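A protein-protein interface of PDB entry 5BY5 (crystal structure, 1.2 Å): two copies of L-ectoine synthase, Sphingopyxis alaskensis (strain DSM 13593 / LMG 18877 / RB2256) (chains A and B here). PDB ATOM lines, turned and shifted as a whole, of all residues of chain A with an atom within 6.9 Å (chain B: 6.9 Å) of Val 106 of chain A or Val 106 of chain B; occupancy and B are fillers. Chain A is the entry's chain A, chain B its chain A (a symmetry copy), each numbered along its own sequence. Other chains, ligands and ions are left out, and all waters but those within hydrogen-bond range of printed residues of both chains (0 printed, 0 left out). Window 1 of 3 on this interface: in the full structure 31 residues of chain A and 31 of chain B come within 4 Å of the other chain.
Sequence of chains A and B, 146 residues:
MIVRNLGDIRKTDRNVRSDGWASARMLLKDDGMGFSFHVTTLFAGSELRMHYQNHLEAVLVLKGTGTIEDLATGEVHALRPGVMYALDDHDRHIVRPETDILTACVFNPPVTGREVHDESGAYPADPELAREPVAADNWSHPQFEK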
ATOM      1  N   MET A  33      18.830  -0.644   0.038  1.00  0.00           N
ATOM      2  CA  MET A  33      18.154  -1.919  -0.083  1.00  0.00           C
ATOM      3  C   MET A  33      16.875  -2.037   0.717  1.00  0.00           C
ATOM      4  O   MET A  33      16.131  -3.016   0.557  1.00  0.00           O
ATOM      5  CB  MET A  33      19.096  -3.057   0.280  1.00  0.00           C
ATOM      6  CG  MET A  33      20.322  -3.177  -0.644  1.00  0.00           C
ATOM      7  SD  MET A  33      19.958  -3.847  -2.268  1.00  0.00           S
ATOM      8  CE  MET A  33      19.703  -5.549  -1.830  1.00  0.00           C
ATOM      9  N   PHE A  35      16.796  -2.571   3.929  1.00  0.00           N
ATOM     10  CA  PHE A  35      17.183  -3.323   5.127  1.00  0.00           C
ATOM     11  C   PHE A  35      18.677  -3.129   5.266  1.00  0.00           C
ATOM     12  O   PHE A  35      19.365  -2.797   4.301  1.00  0.00           O
ATOM     13  CB  PHE A  35      16.833  -4.833   5.014  1.00  0.00           C
ATOM     14  CG  PHE A  35      17.456  -5.542   3.852  1.00  0.00           C
ATOM     15  CD1 PHE A  35      18.715  -6.099   3.940  1.00  0.00           C
ATOM     16  CD2 PHE A  35      16.808  -5.640   2.653  1.00  0.00           C
ATOM     17  CE1 PHE A  35      19.291  -6.782   2.871  1.00  0.00           C
ATOM     18  CE2 PHE A  35      17.348  -6.307   1.560  1.00  0.00           C
ATOM     19  CZ  PHE A  35      18.588  -6.879   1.678  1.00  0.00           C
ATOM     20  N   SER A  36      19.173  -3.338   6.485  1.00  0.00           N
ATOM     21  CA  SER A  36      20.606  -3.362   6.743  1.00  0.00           C
ATOM     22  C   SER A  36      21.058  -4.787   6.992  1.00  0.00           C
ATOM     23  O   SER A  36      20.240  -5.628   7.388  1.00  0.00           O
ATOM     24  CB  SER A  36      21.030  -2.380   7.825  1.00  0.00           C
ATOM     25  OG  SER A  36      20.419  -2.684   9.065  1.00  0.00           O
ATOM     26  N   PHE A  37      22.330  -5.073   6.744  1.00  0.00           N
ATOM     27  CA  PHE A  37      22.859  -6.439   6.773  1.00  0.00           C
ATOM     28  C   PHE A  37      24.220  -6.388   7.400  1.00  0.00           C
ATOM     29  O   PHE A  37      25.108  -5.696   6.919  1.00  0.00           O
ATOM     30  CB  PHE A  37      22.891  -7.008   5.352  1.00  0.00           C
ATOM     31  CG  PHE A  37      22.980  -8.517   5.176  1.00  0.00           C
ATOM     32  CD1 PHE A  37      22.643  -9.450   6.106  1.00  0.00           C
ATOM     33  CD2 PHE A  37      23.293  -9.014   3.924  1.00  0.00           C
ATOM     34  CE1 PHE A  37      22.681 -10.808   5.834  1.00  0.00           C
ATOM     35  CE2 PHE A  37      23.316 -10.359   3.656  1.00  0.00           C
ATOM     36  CZ  PHE A  37      22.970 -11.285   4.605  1.00  0.00           C
ATOM     37  N   HIS A  38      24.363  -7.056   8.523  1.00  0.00           N
ATOM     38  CA  HIS A  38      25.523  -6.944   9.400  1.00  0.00           C
ATOM     39  C   HIS A  38      26.125  -8.312   9.672  1.00  0.00           C
ATOM     40  O   HIS A  38      25.379  -9.302   9.789  1.00  0.00           O
ATOM     41  CB  HIS A  38      25.134  -6.354  10.747  1.00  0.00           C
ATOM     42  CG  HIS A  38      24.206  -5.153  10.728  1.00  0.00           C
ATOM     43  ND1 HIS A  38      24.305  -4.142  11.612  1.00  0.00           N
ATOM     44  CD2 HIS A  38      23.108  -4.824  10.018  1.00  0.00           C
ATOM     45  CE1 HIS A  38      23.374  -3.224  11.420  1.00  0.00           C
ATOM     46  NE2 HIS A  38      22.681  -3.571  10.388  1.00  0.00           N
ATOM     47  N   LEU A  56      12.724  -4.188  13.379  1.00  0.00           N
ATOM     48  CA  LEU A  56      12.652  -5.642  13.373  1.00  0.00           C
ATOM     49  C   LEU A  56      14.064  -6.171  13.085  1.00  0.00           C
ATOM     50  O   LEU A  56      14.762  -5.598  12.248  1.00  0.00           O
ATOM     51  CB  LEU A  56      11.643  -6.136  12.313  1.00  0.00           C
ATOM     52  CG  LEU A  56      10.245  -5.594  12.449  1.00  0.00           C
ATOM     53  CD1 LEU A  56       9.369  -6.035  11.296  1.00  0.00           C
ATOM     54  CD2 LEU A  56       9.619  -6.010  13.759  1.00  0.00           C
ATOM     55  N   GLU A  57      14.442  -7.265  13.712  1.00  0.00           N
ATOM     56  CA  GLU A  57      15.767  -7.850  13.512  1.00  0.00           C
ATOM     57  C   GLU A  57      15.657  -9.365  13.355  1.00  0.00           C
ATOM     58  O   GLU A  57      14.973 -10.007  14.145  1.00  0.00           O
ATOM     59  CB  GLU A  57      16.730  -7.539  14.676  1.00  0.00           C
ATOM     60  CG  GLU A  57      18.203  -7.995  14.299  1.00  0.00           C
ATOM     61  CD  GLU A  57      19.236  -8.012  15.405  1.00  0.00           C
ATOM     62  OE1 GLU A  57      18.894  -7.795  16.578  1.00  0.00           O
ATOM     63  OE2 GLU A  57      20.455  -8.223  15.028  1.00  0.00           O
ATOM     64  N   ALA A  58      16.359  -9.913  12.380  1.00  0.00           N
ATOM     65  CA  ALA A  58      16.581 -11.348  12.278  1.00  0.00           C
ATOM     66  C   ALA A  58      18.070 -11.614  12.406  1.00  0.00           C
ATOM     67  O   ALA A  58      18.891 -10.861  11.879  1.00  0.00           O
ATOM     68  CB  ALA A  58      16.072 -11.907  10.967  1.00  0.00           C
ATOM     69  N   VAL A  59      18.394 -12.705  13.065  1.00  0.00           N
ATOM     70  CA  VAL A  59      19.764 -13.094  13.378  1.00  0.00           C
ATOM     71  C   VAL A  59      19.981 -14.555  13.086  1.00  0.00           C
ATOM     72  O   VAL A  59      19.257 -15.390  13.620  1.00  0.00           O
ATOM     73  CB  VAL A  59      20.071 -12.831  14.864  1.00  0.00           C
ATOM     74  CG1 VAL A  59      21.502 -13.230  15.176  1.00  0.00           C
ATOM     75  CG2 VAL A  59      19.812 -11.375  15.202  1.00  0.00           C
ATOM     76  N   LEU A  60      20.938 -14.867  12.213  1.00  0.00           N
ATOM     77  CA  LEU A  60      21.330 -16.224  11.932  1.00  0.00           C
ATOM     78  C   LEU A  60      22.680 -16.499  12.579  1.00  0.00           C
ATOM     79  O   LEU A  60      23.643 -15.817  12.292  1.00  0.00           O
ATOM     80  CB  LEU A  60      21.429 -16.481  10.431  1.00  0.00           C
ATOM     81  CG  LEU A  60      21.860 -17.861   9.996  1.00  0.00           C
ATOM     82  CD1 LEU A  60      20.871 -18.920  10.370  1.00  0.00           C
ATOM     83  CD2 LEU A  60      22.133 -17.887   8.511  1.00  0.00           C
ATOM     84  N   ALA A 104      24.903 -13.384  11.229  1.00  0.00           N
ATOM     85  CA  ALA A 104      24.439 -12.554  10.133  1.00  0.00           C
ATOM     86  C   ALA A 104      23.097 -11.955  10.550  1.00  0.00           C
ATOM     87  O   ALA A 104      22.194 -12.693  10.902  1.00  0.00           O
ATOM     88  CB  ALA A 104      24.294 -13.331   8.844  1.00  0.00           C
ATOM     89  N   CYS A 105      22.993 -10.625  10.541  1.00  0.00           N
ATOM     90  CA  CYS A 105      21.860  -9.930  11.106  1.00  0.00           C
ATOM     91  C   CYS A 105      21.230  -9.030  10.054  1.00  0.00           C
ATOM     92  O   CYS A 105      21.940  -8.351   9.310  1.00  0.00           O
ATOM     93  CB  CYS A 105      22.281  -9.064  12.285  1.00  0.00           C
ATOM     94  SG  CYS A 105      23.108  -9.933  13.587  1.00  0.00           S
ATOM     95  N   VAL A 106      19.911  -8.944  10.083  1.00  0.00           N
ATOM     96  CA  VAL A 106      19.130  -8.117   9.178  1.00  0.00           C
ATOM     97  C   VAL A 106      18.216  -7.238  10.003  1.00  0.00           C
ATOM     98  O   VAL A 106      17.546  -7.729  10.870  1.00  0.00           O
ATOM     99  CB  VAL A 106      18.253  -8.990   8.234  1.00  0.00           C
ATOM    100  CG1 VAL A 106      17.522  -8.099   7.252  1.00  0.00           C
ATOM    101  CG2 VAL A 106      19.087 -10.053   7.549  1.00  0.00           C
ATOM    102  N   PHE A 107      18.200  -5.944   9.684  1.00  0.00           N
ATOM    103  CA  PHE A 107      17.290  -4.999  10.328  1.00  0.00           C
ATOM    104  C   PHE A 107      16.381  -4.365   9.292  1.00  0.00           C
ATOM    105  O   PHE A 107      16.821  -3.964   8.202  1.00  0.00           O
ATOM    106  CB  PHE A 107      18.024  -3.867  11.049  1.00  0.00           C
ATOM    107  CG  PHE A 107      18.773  -4.302  12.277  1.00  0.00           C
ATOM    108  CD1 PHE A 107      20.035  -4.885  12.146  1.00  0.00           C
ATOM    109  CD2 PHE A 107      18.263  -4.106  13.538  1.00  0.00           C
ATOM    110  CE1 PHE A 107      20.772  -5.275  13.249  1.00  0.00           C
ATOM    111  CE2 PHE A 107      18.981  -4.473  14.646  1.00  0.00           C
ATOM    112  CZ  PHE A 107      20.236  -5.069  14.483  1.00  0.00           C
ATOM    113  N   ASN A 108      15.099  -4.236   9.664  1.00  0.00           N
ATOM    114  CA  ASN A 108      14.100  -3.534   8.886  1.00  0.00           C
ATOM    115  C   ASN A 108      13.301  -2.656   9.826  1.00  0.00           C
ATOM    116  O   ASN A 108      12.686  -3.191  10.743  1.00  0.00           O
ATOM    117  CB  ASN A 108      13.166  -4.529   8.214  1.00  0.00           C
ATOM    118  CG  ASN A 108      12.081  -3.873   7.428  1.00  0.00           C
ATOM    119  OD1 ASN A 108      12.254  -2.756   6.951  1.00  0.00           O
ATOM    120  ND2 ASN A 108      11.022  -4.586   7.191  1.00  0.00           N
ATOM    121  N   PRO A 109      13.268  -1.331   9.623  1.00  0.00           N
ATOM    122  CA  PRO A 109      13.993  -0.582   8.600  1.00  0.00           C
ATOM    123  C   PRO A 109      15.489  -0.691   8.824  1.00  0.00           C
ATOM    124  O   PRO A 109      15.954  -1.143   9.857  1.00  0.00           O
ATOM    125  CB  PRO A 109      13.487   0.847   8.809  1.00  0.00           C
ATOM    126  CG  PRO A 109      12.309   0.749   9.637  1.00  0.00           C
ATOM    127  CD  PRO A 109      12.455  -0.446  10.472  1.00  0.00           C
ATOM    128  N   MET B  33       8.061 -10.027   8.742  1.00  0.00           N
ATOM    129  CA  MET B  33       9.220  -9.193   8.985  1.00  0.00           C
ATOM    130  C   MET B  33       9.476  -8.142   7.927  1.00  0.00           C
ATOM    131  O   MET B  33      10.337  -7.269   8.116  1.00  0.00           O
ATOM    132  CB  MET B  33      10.461 -10.050   9.174  1.00  0.00           C
ATOM    133  CG  MET B  33      10.397 -10.991  10.391  1.00  0.00           C
ATOM    134  SD  MET B  33      10.590 -10.165  11.972  1.00  0.00           S
ATOM    135  CE  MET B  33      12.330  -9.820  11.909  1.00  0.00           C
ATOM    136  N   PHE B  35      10.842  -8.783   5.040  1.00  0.00           N
ATOM    137  CA  PHE B  35      11.905  -9.356   4.208  1.00  0.00           C
ATOM    138  C   PHE B  35      11.836 -10.850   4.429  1.00  0.00           C
ATOM    139  O   PHE B  35      11.296 -11.319   5.432  1.00  0.00           O
ATOM    140  CB  PHE B  35      13.310  -8.808   4.587  1.00  0.00           C
ATOM    141  CG  PHE B  35      13.717  -9.039   6.009  1.00  0.00           C
ATOM    142  CD1 PHE B  35      14.343 -10.206   6.398  1.00  0.00           C
ATOM    143  CD2 PHE B  35      13.456  -8.113   6.980  1.00  0.00           C
ATOM    144  CE1 PHE B  35      14.748 -10.417   7.714  1.00  0.00           C
ATOM    145  CE2 PHE B  35      13.836  -8.286   8.305  1.00  0.00           C
ATOM    146  CZ  PHE B  35      14.485  -9.439   8.664  1.00  0.00           C
ATOM    147  N   SER B  36      12.388 -11.599   3.475  1.00  0.00           N
ATOM    148  CA  SER B  36      12.557 -13.039   3.622  1.00  0.00           C
ATOM    149  C   SER B  36      14.019 -13.361   3.856  1.00  0.00           C
ATOM    150  O   SER B  36      14.890 -12.569   3.474  1.00  0.00           O
ATOM    151  CB  SER B  36      11.922 -13.828   2.486  1.00  0.00           C
ATOM    152  OG  SER B  36      12.512 -13.505   1.241  1.00  0.00           O
ATOM    153  N   PHE B  37      14.297 -14.491   4.495  1.00  0.00           N
ATOM    154  CA  PHE B  37      15.647 -14.842   4.941  1.00  0.00           C
ATOM    155  C   PHE B  37      15.838 -16.310   4.706  1.00  0.00           C
ATOM    156  O   PHE B  37      15.092 -17.131   5.223  1.00  0.00           O
ATOM    157  CB  PHE B  37      15.820 -14.458   6.413  1.00  0.00           C
ATOM    158  CG  PHE B  37      17.229 -14.319   6.968  1.00  0.00           C
ATOM    159  CD1 PHE B  37      18.356 -14.107   6.238  1.00  0.00           C
ATOM    160  CD2 PHE B  37      17.391 -14.255   8.340  1.00  0.00           C
ATOM    161  CE1 PHE B  37      19.593 -13.913   6.832  1.00  0.00           C
ATOM    162  CE2 PHE B  37      18.614 -14.049   8.923  1.00  0.00           C
ATOM    163  CZ  PHE B  37      19.741 -13.836   8.171  1.00  0.00           C
ATOM    164  N   HIS B  38      16.788 -16.639   3.859  1.00  0.00           N
ATOM    165  CA  HIS B  38      16.975 -17.983   3.323  1.00  0.00           C
ATOM    166  C   HIS B  38      18.397 -18.462   3.562  1.00  0.00           C
ATOM    167  O   HIS B  38      19.341 -17.654   3.494  1.00  0.00           O
ATOM    168  CB  HIS B  38      16.745 -18.008   1.819  1.00  0.00           C
ATOM    169  CG  HIS B  38      15.535 -17.255   1.298  1.00  0.00           C
ATOM    170  ND1 HIS B  38      14.803 -17.687   0.254  1.00  0.00           N
ATOM    171  CD2 HIS B  38      14.971 -16.066   1.588  1.00  0.00           C
ATOM    172  CE1 HIS B  38      13.817 -16.856  -0.038  1.00  0.00           C
ATOM    173  NE2 HIS B  38      13.839 -15.896   0.825  1.00  0.00           N
ATOM    174  N   LEU B  56      14.694  -6.966  -4.466  1.00  0.00           N
ATOM    175  CA  LEU B  56      16.089  -6.719  -4.125  1.00  0.00           C
ATOM    176  C   LEU B  56      16.597  -7.944  -3.353  1.00  0.00           C
ATOM    177  O   LEU B  56      15.861  -8.482  -2.525  1.00  0.00           O
ATOM    178  CB  LEU B  56      16.228  -5.430  -3.286  1.00  0.00           C
ATOM    179  CG  LEU B  56      15.667  -4.183  -3.916  1.00  0.00           C
ATOM    180  CD1 LEU B  56      15.737  -3.006  -2.966  1.00  0.00           C
ATOM    181  CD2 LEU B  56      16.383  -3.849  -5.204  1.00  0.00           C
ATOM    182  N   GLU B  57      17.837  -8.328  -3.571  1.00  0.00           N
ATOM    183  CA  GLU B  57      18.417  -9.484  -2.889  1.00  0.00           C
ATOM    184  C   GLU B  57      19.828  -9.156  -2.404  1.00  0.00           C
ATOM    185  O   GLU B  57      20.620  -8.612  -3.167  1.00  0.00           O
ATOM    186  CB  GLU B  57      18.480 -10.731  -3.795  1.00  0.00           C
ATOM    187  CG  GLU B  57      18.897 -12.001  -2.939  1.00  0.00           C
ATOM    188  CD  GLU B  57      19.264 -13.263  -3.693  1.00  0.00           C
ATOM    189  OE1 GLU B  57      19.349 -13.245  -4.930  1.00  0.00           O
ATOM    190  OE2 GLU B  57      19.432 -14.320  -2.965  1.00  0.00           O
ATOM    191  N   ALA B  58      20.134  -9.529  -1.174  1.00  0.00           N
ATOM    192  CA  ALA B  58      21.500  -9.544  -0.672  1.00  0.00           C
ATOM    193  C   ALA B  58      21.870 -10.976  -0.330  1.00  0.00           C
ATOM    194  O   ALA B  58      21.049 -11.729   0.197  1.00  0.00           O
ATOM    195  CB  ALA B  58      21.661  -8.667   0.552  1.00  0.00           C
ATOM    196  N   VAL B  59      23.113 -11.315  -0.593  1.00  0.00           N
ATOM    197  CA  VAL B  59      23.643 -12.663  -0.426  1.00  0.00           C
ATOM    198  C   VAL B  59      24.983 -12.624   0.260  1.00  0.00           C
ATOM    199  O   VAL B  59      25.891 -11.957  -0.228  1.00  0.00           O
ATOM    200  CB  VAL B  59      23.804 -13.352  -1.794  1.00  0.00           C
ATOM    201  CG1 VAL B  59      24.347 -14.756  -1.607  1.00  0.00           C
ATOM    202  CG2 VAL B  59      22.477 -13.362  -2.532  1.00  0.00           C
ATOM    203  N   LEU B  60      25.104 -13.296   1.405  1.00  0.00           N
ATOM    204  CA  LEU B  60      26.356 -13.440   2.100  1.00  0.00           C
ATOM    205  C   LEU B  60      26.866 -14.864   1.923  1.00  0.00           C
ATOM    206  O   LEU B  60      26.185 -15.803   2.282  1.00  0.00           O
ATOM    207  CB  LEU B  60      26.209 -13.140   3.590  1.00  0.00           C
ATOM    208  CG  LEU B  60      27.444 -13.282   4.446  1.00  0.00           C
ATOM    209  CD1 LEU B  60      28.510 -12.292   4.091  1.00  0.00           C
ATOM    210  CD2 LEU B  60      27.089 -13.181   5.910  1.00  0.00           C
ATOM    211  N   ALA B 104      23.627 -17.052   3.018  1.00  0.00           N
ATOM    212  CA  ALA B 104      22.512 -16.439   3.714  1.00  0.00           C
ATOM    213  C   ALA B 104      21.974 -15.321   2.822  1.00  0.00           C
ATOM    214  O   ALA B 104      22.729 -14.449   2.434  1.00  0.00           O
ATOM    215  CB  ALA B 104      22.909 -15.892   5.066  1.00  0.00           C
ATOM    216  N   CYS B 105      20.686 -15.380   2.480  1.00  0.00           N
ATOM    217  CA  CYS B 105      20.107 -14.511   1.482  1.00  0.00           C
ATOM    218  C   CYS B 105      18.927 -13.758   2.078  1.00  0.00           C
ATOM    219  O   CYS B 105      18.114 -14.342   2.795  1.00  0.00           O
ATOM    220  CB  CYS B 105      19.610 -15.308   0.284  1.00  0.00           C
ATOM    221  SG  CYS B 105      20.837 -16.315  -0.499  1.00  0.00           S
ATOM    222  N   VAL B 106      18.780 -12.506   1.678  1.00  0.00           N
ATOM    223  CA  VAL B 106      17.702 -11.635   2.114  1.00  0.00           C
ATOM    224  C   VAL B 106      17.027 -11.062   0.887  1.00  0.00           C
ATOM    225  O   VAL B 106      17.694 -10.568   0.019  1.00  0.00           O
ATOM    226  CB  VAL B 106      18.243 -10.455   2.973  1.00  0.00           C
ATOM    227  CG1 VAL B 106      17.086  -9.620   3.477  1.00  0.00           C
ATOM    228  CG2 VAL B 106      19.129 -10.962   4.092  1.00  0.00           C
ATOM    229  N   PHE B 107      15.695 -11.125   0.866  1.00  0.00           N
ATOM    230  CA  PHE B 107      14.908 -10.520  -0.208  1.00  0.00           C
ATOM    231  C   PHE B 107      13.973  -9.470   0.363  1.00  0.00           C
ATOM    232  O   PHE B 107      13.321  -9.678   1.399  1.00  0.00           O
ATOM    233  CB  PHE B 107      14.050 -11.539  -0.960  1.00  0.00           C
ATOM    234  CG  PHE B 107      14.836 -12.506  -1.800  1.00  0.00           C
ATOM    235  CD1 PHE B 107      15.430 -13.618  -1.200  1.00  0.00           C
ATOM    236  CD2 PHE B 107      14.956 -12.345  -3.160  1.00  0.00           C
ATOM    237  CE1 PHE B 107      16.138 -14.548  -1.938  1.00  0.00           C
ATOM    238  CE2 PHE B 107      15.642 -13.261  -3.913  1.00  0.00           C
ATOM    239  CZ  PHE B 107      16.240 -14.357  -3.281  1.00  0.00           C
ATOM    240  N   ASN B 108      13.880  -8.343  -0.356  1.00  0.00           N
ATOM    241  CA  ASN B 108      12.943  -7.277  -0.068  1.00  0.00           C
ATOM    242  C   ASN B 108      12.305  -6.842  -1.370  1.00  0.00           C
ATOM    243  O   ASN B 108      13.032  -6.409  -2.260  1.00  0.00           O
ATOM    244  CB  ASN B 108      13.672  -6.094   0.552  1.00  0.00           C
ATOM    245  CG  ASN B 108      12.773  -4.938   0.837  1.00  0.00           C
ATOM    246  OD1 ASN B 108      11.580  -5.124   1.057  1.00  0.00           O
ATOM    247  ND2 ASN B 108      13.339  -3.775   0.950  1.00  0.00           N
ATOM    248  N   PRO B 109      10.974  -6.921  -1.512  1.00  0.00           N
ATOM    249  CA  PRO B 109      10.021  -7.462  -0.547  1.00  0.00           C
ATOM    250  C   PRO B 109      10.266  -8.943  -0.330  1.00  0.00           C
ATOM    251  O   PRO B 109      11.000  -9.587  -1.061  1.00  0.00           O
ATOM    252  CB  PRO B 109       8.673  -7.199  -1.224  1.00  0.00           C
ATOM    253  CG  PRO B 109       8.925  -6.254  -2.286  1.00  0.00           C
ATOM    254  CD  PRO B 109      10.305  -6.453  -2.735  1.00  0.00           C
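Met 33 of chain A touches Leu 56 of chain B (O to CD1, 3.5 Å). CG1 of Val 106 of chain B touches CZ of Phe 35 of chain A, at 3.6 Å. Phe 37 of chain A touches Ala 58 of chain B (CD2 to CB, 3.8 Å). Phe 37 of chain A touches Ala 104 of chain B (CZ to O, 3.8 Å). Val 106 of chain B touches Phe 37 of chain A (CG2 to CZ, 3.9 Å). CD1 of Leu 56 of chain A touches O of Met 33 of chain B (3.5 Å). O of Glu 57 of chain A touches CE of Met 33 of chain B, 3.5 Å away. CZ of Phe 35 of chain B touches CB of Ala 58 of chain A, at 3.7 Å. CD2 of Phe 37 of chain B touches CB of Ala 58 of chain A (3.8 Å). Val 106 of chain A touches Phe 35 of chain B (CG1 to CZ, 3.6 Å).
O of Met 33 of chain A lies within hydrogen-bond range of ND2 of Asn 108 of chain B (2.9 Å). The backbone carbonyl oxygen of Met 33 of chain B sits at hydrogen-bond distance from the side-chain amide nitrogen of Asn 108 of chain A, 2.9 Å away.
Hydrophobic or aromatic side chains of chain B within 4 Å of the printed part of chain A: Met 33, Phe 35, Phe 37, Leu 56, Ala 58, Leu 60 and Val 106. Of the 16 printed residues of chain A, 10 touch a printed residue of chain B. Hydrophobic or aromatic side chains of chain A that line the printed part of chain B: Met 33, Phe 35, Phe 37, Leu 56, Ala 58, Leu 60 and Val 106. Among the printed residues, 21 pairs touch across the chains. Among the printed residues, no Asp or Glu carboxylate lies within 4 Å of a Lys or Arg side-chain nitrogen of the other chain.
N of Leu 56 of chain A lies within hydrogen-bond range of O of Asn 108 of chain A. The backbone NH of Leu 60 of chain A lies within hydrogen-bond range of the backbone carbonyl oxygen of Ala 104 of chain A (2.8 Å). The backbone NH (N) of Leu 56 of chain B lies within hydrogen-bond range of the backbone carbonyl oxygen (O) of Asn 108 of chain B, at 2.8 Å. The side-chain carboxylate of Glu 57 of chain B sits close to the side-chain sulfur of Cys 105 of chain B (3.5 Å). The backbone carbonyl oxygen (O) of Ala 58 of chain B lies within hydrogen-bond range of the backbone NH (N) of Val 106 of chain B (2.8 Å). The backbone NH (N) of Leu 60 of chain B sits at hydrogen-bond distance from the backbone carbonyl oxygen (O) of Ala 104 of chain B.
Of chain B, only Phe 35, Phe 37 and Val 106 come within 4 Å of Val 106 of chain A. Val 106 of chain B touches three residues of chain A. Of the printed residues of chain A, Leu 60 of chain B touches Phe 37 (3.9 Å). Of the printed residues of chain A, Glu 57 of chain B touches Met 33 (3.5 Å). Of the printed residues of chain B, Ala 104 of chain A touches Phe 37 (3.8 Å). The nearest residue of chain A that does not touch Val 106 of chain B is Met 33 of chain A (5.7 Å). The nearest printed residue of chain B that does not touch Asn 108 of chain A is Asn 108 of chain B (6.2 Å).
Phe 35 of chain A touches Ala 58 of chain B, and with the chains exchanged Ala 58 of chain A touches Phe 35 of chain B. Phe 35 of chain A touches Val 106 of chain B, and with the chains exchanged Val 106 of chain A touches Phe 35 of chain B. Phe 37 of chain A touches Ala 104 of chain B, and with the chains exchanged Ala 104 of chain A touches Phe 37 of chain B. Phe 37 of chain A touches Val 106 of chain B, and with the chains exchanged Val 106 of chain A touches Phe 37 of chain B. 16 positions are printed for both chains. Of the 21 pairs that touch across the chains among the printed residues, 21 have their exchanged pair printed and touching as well.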
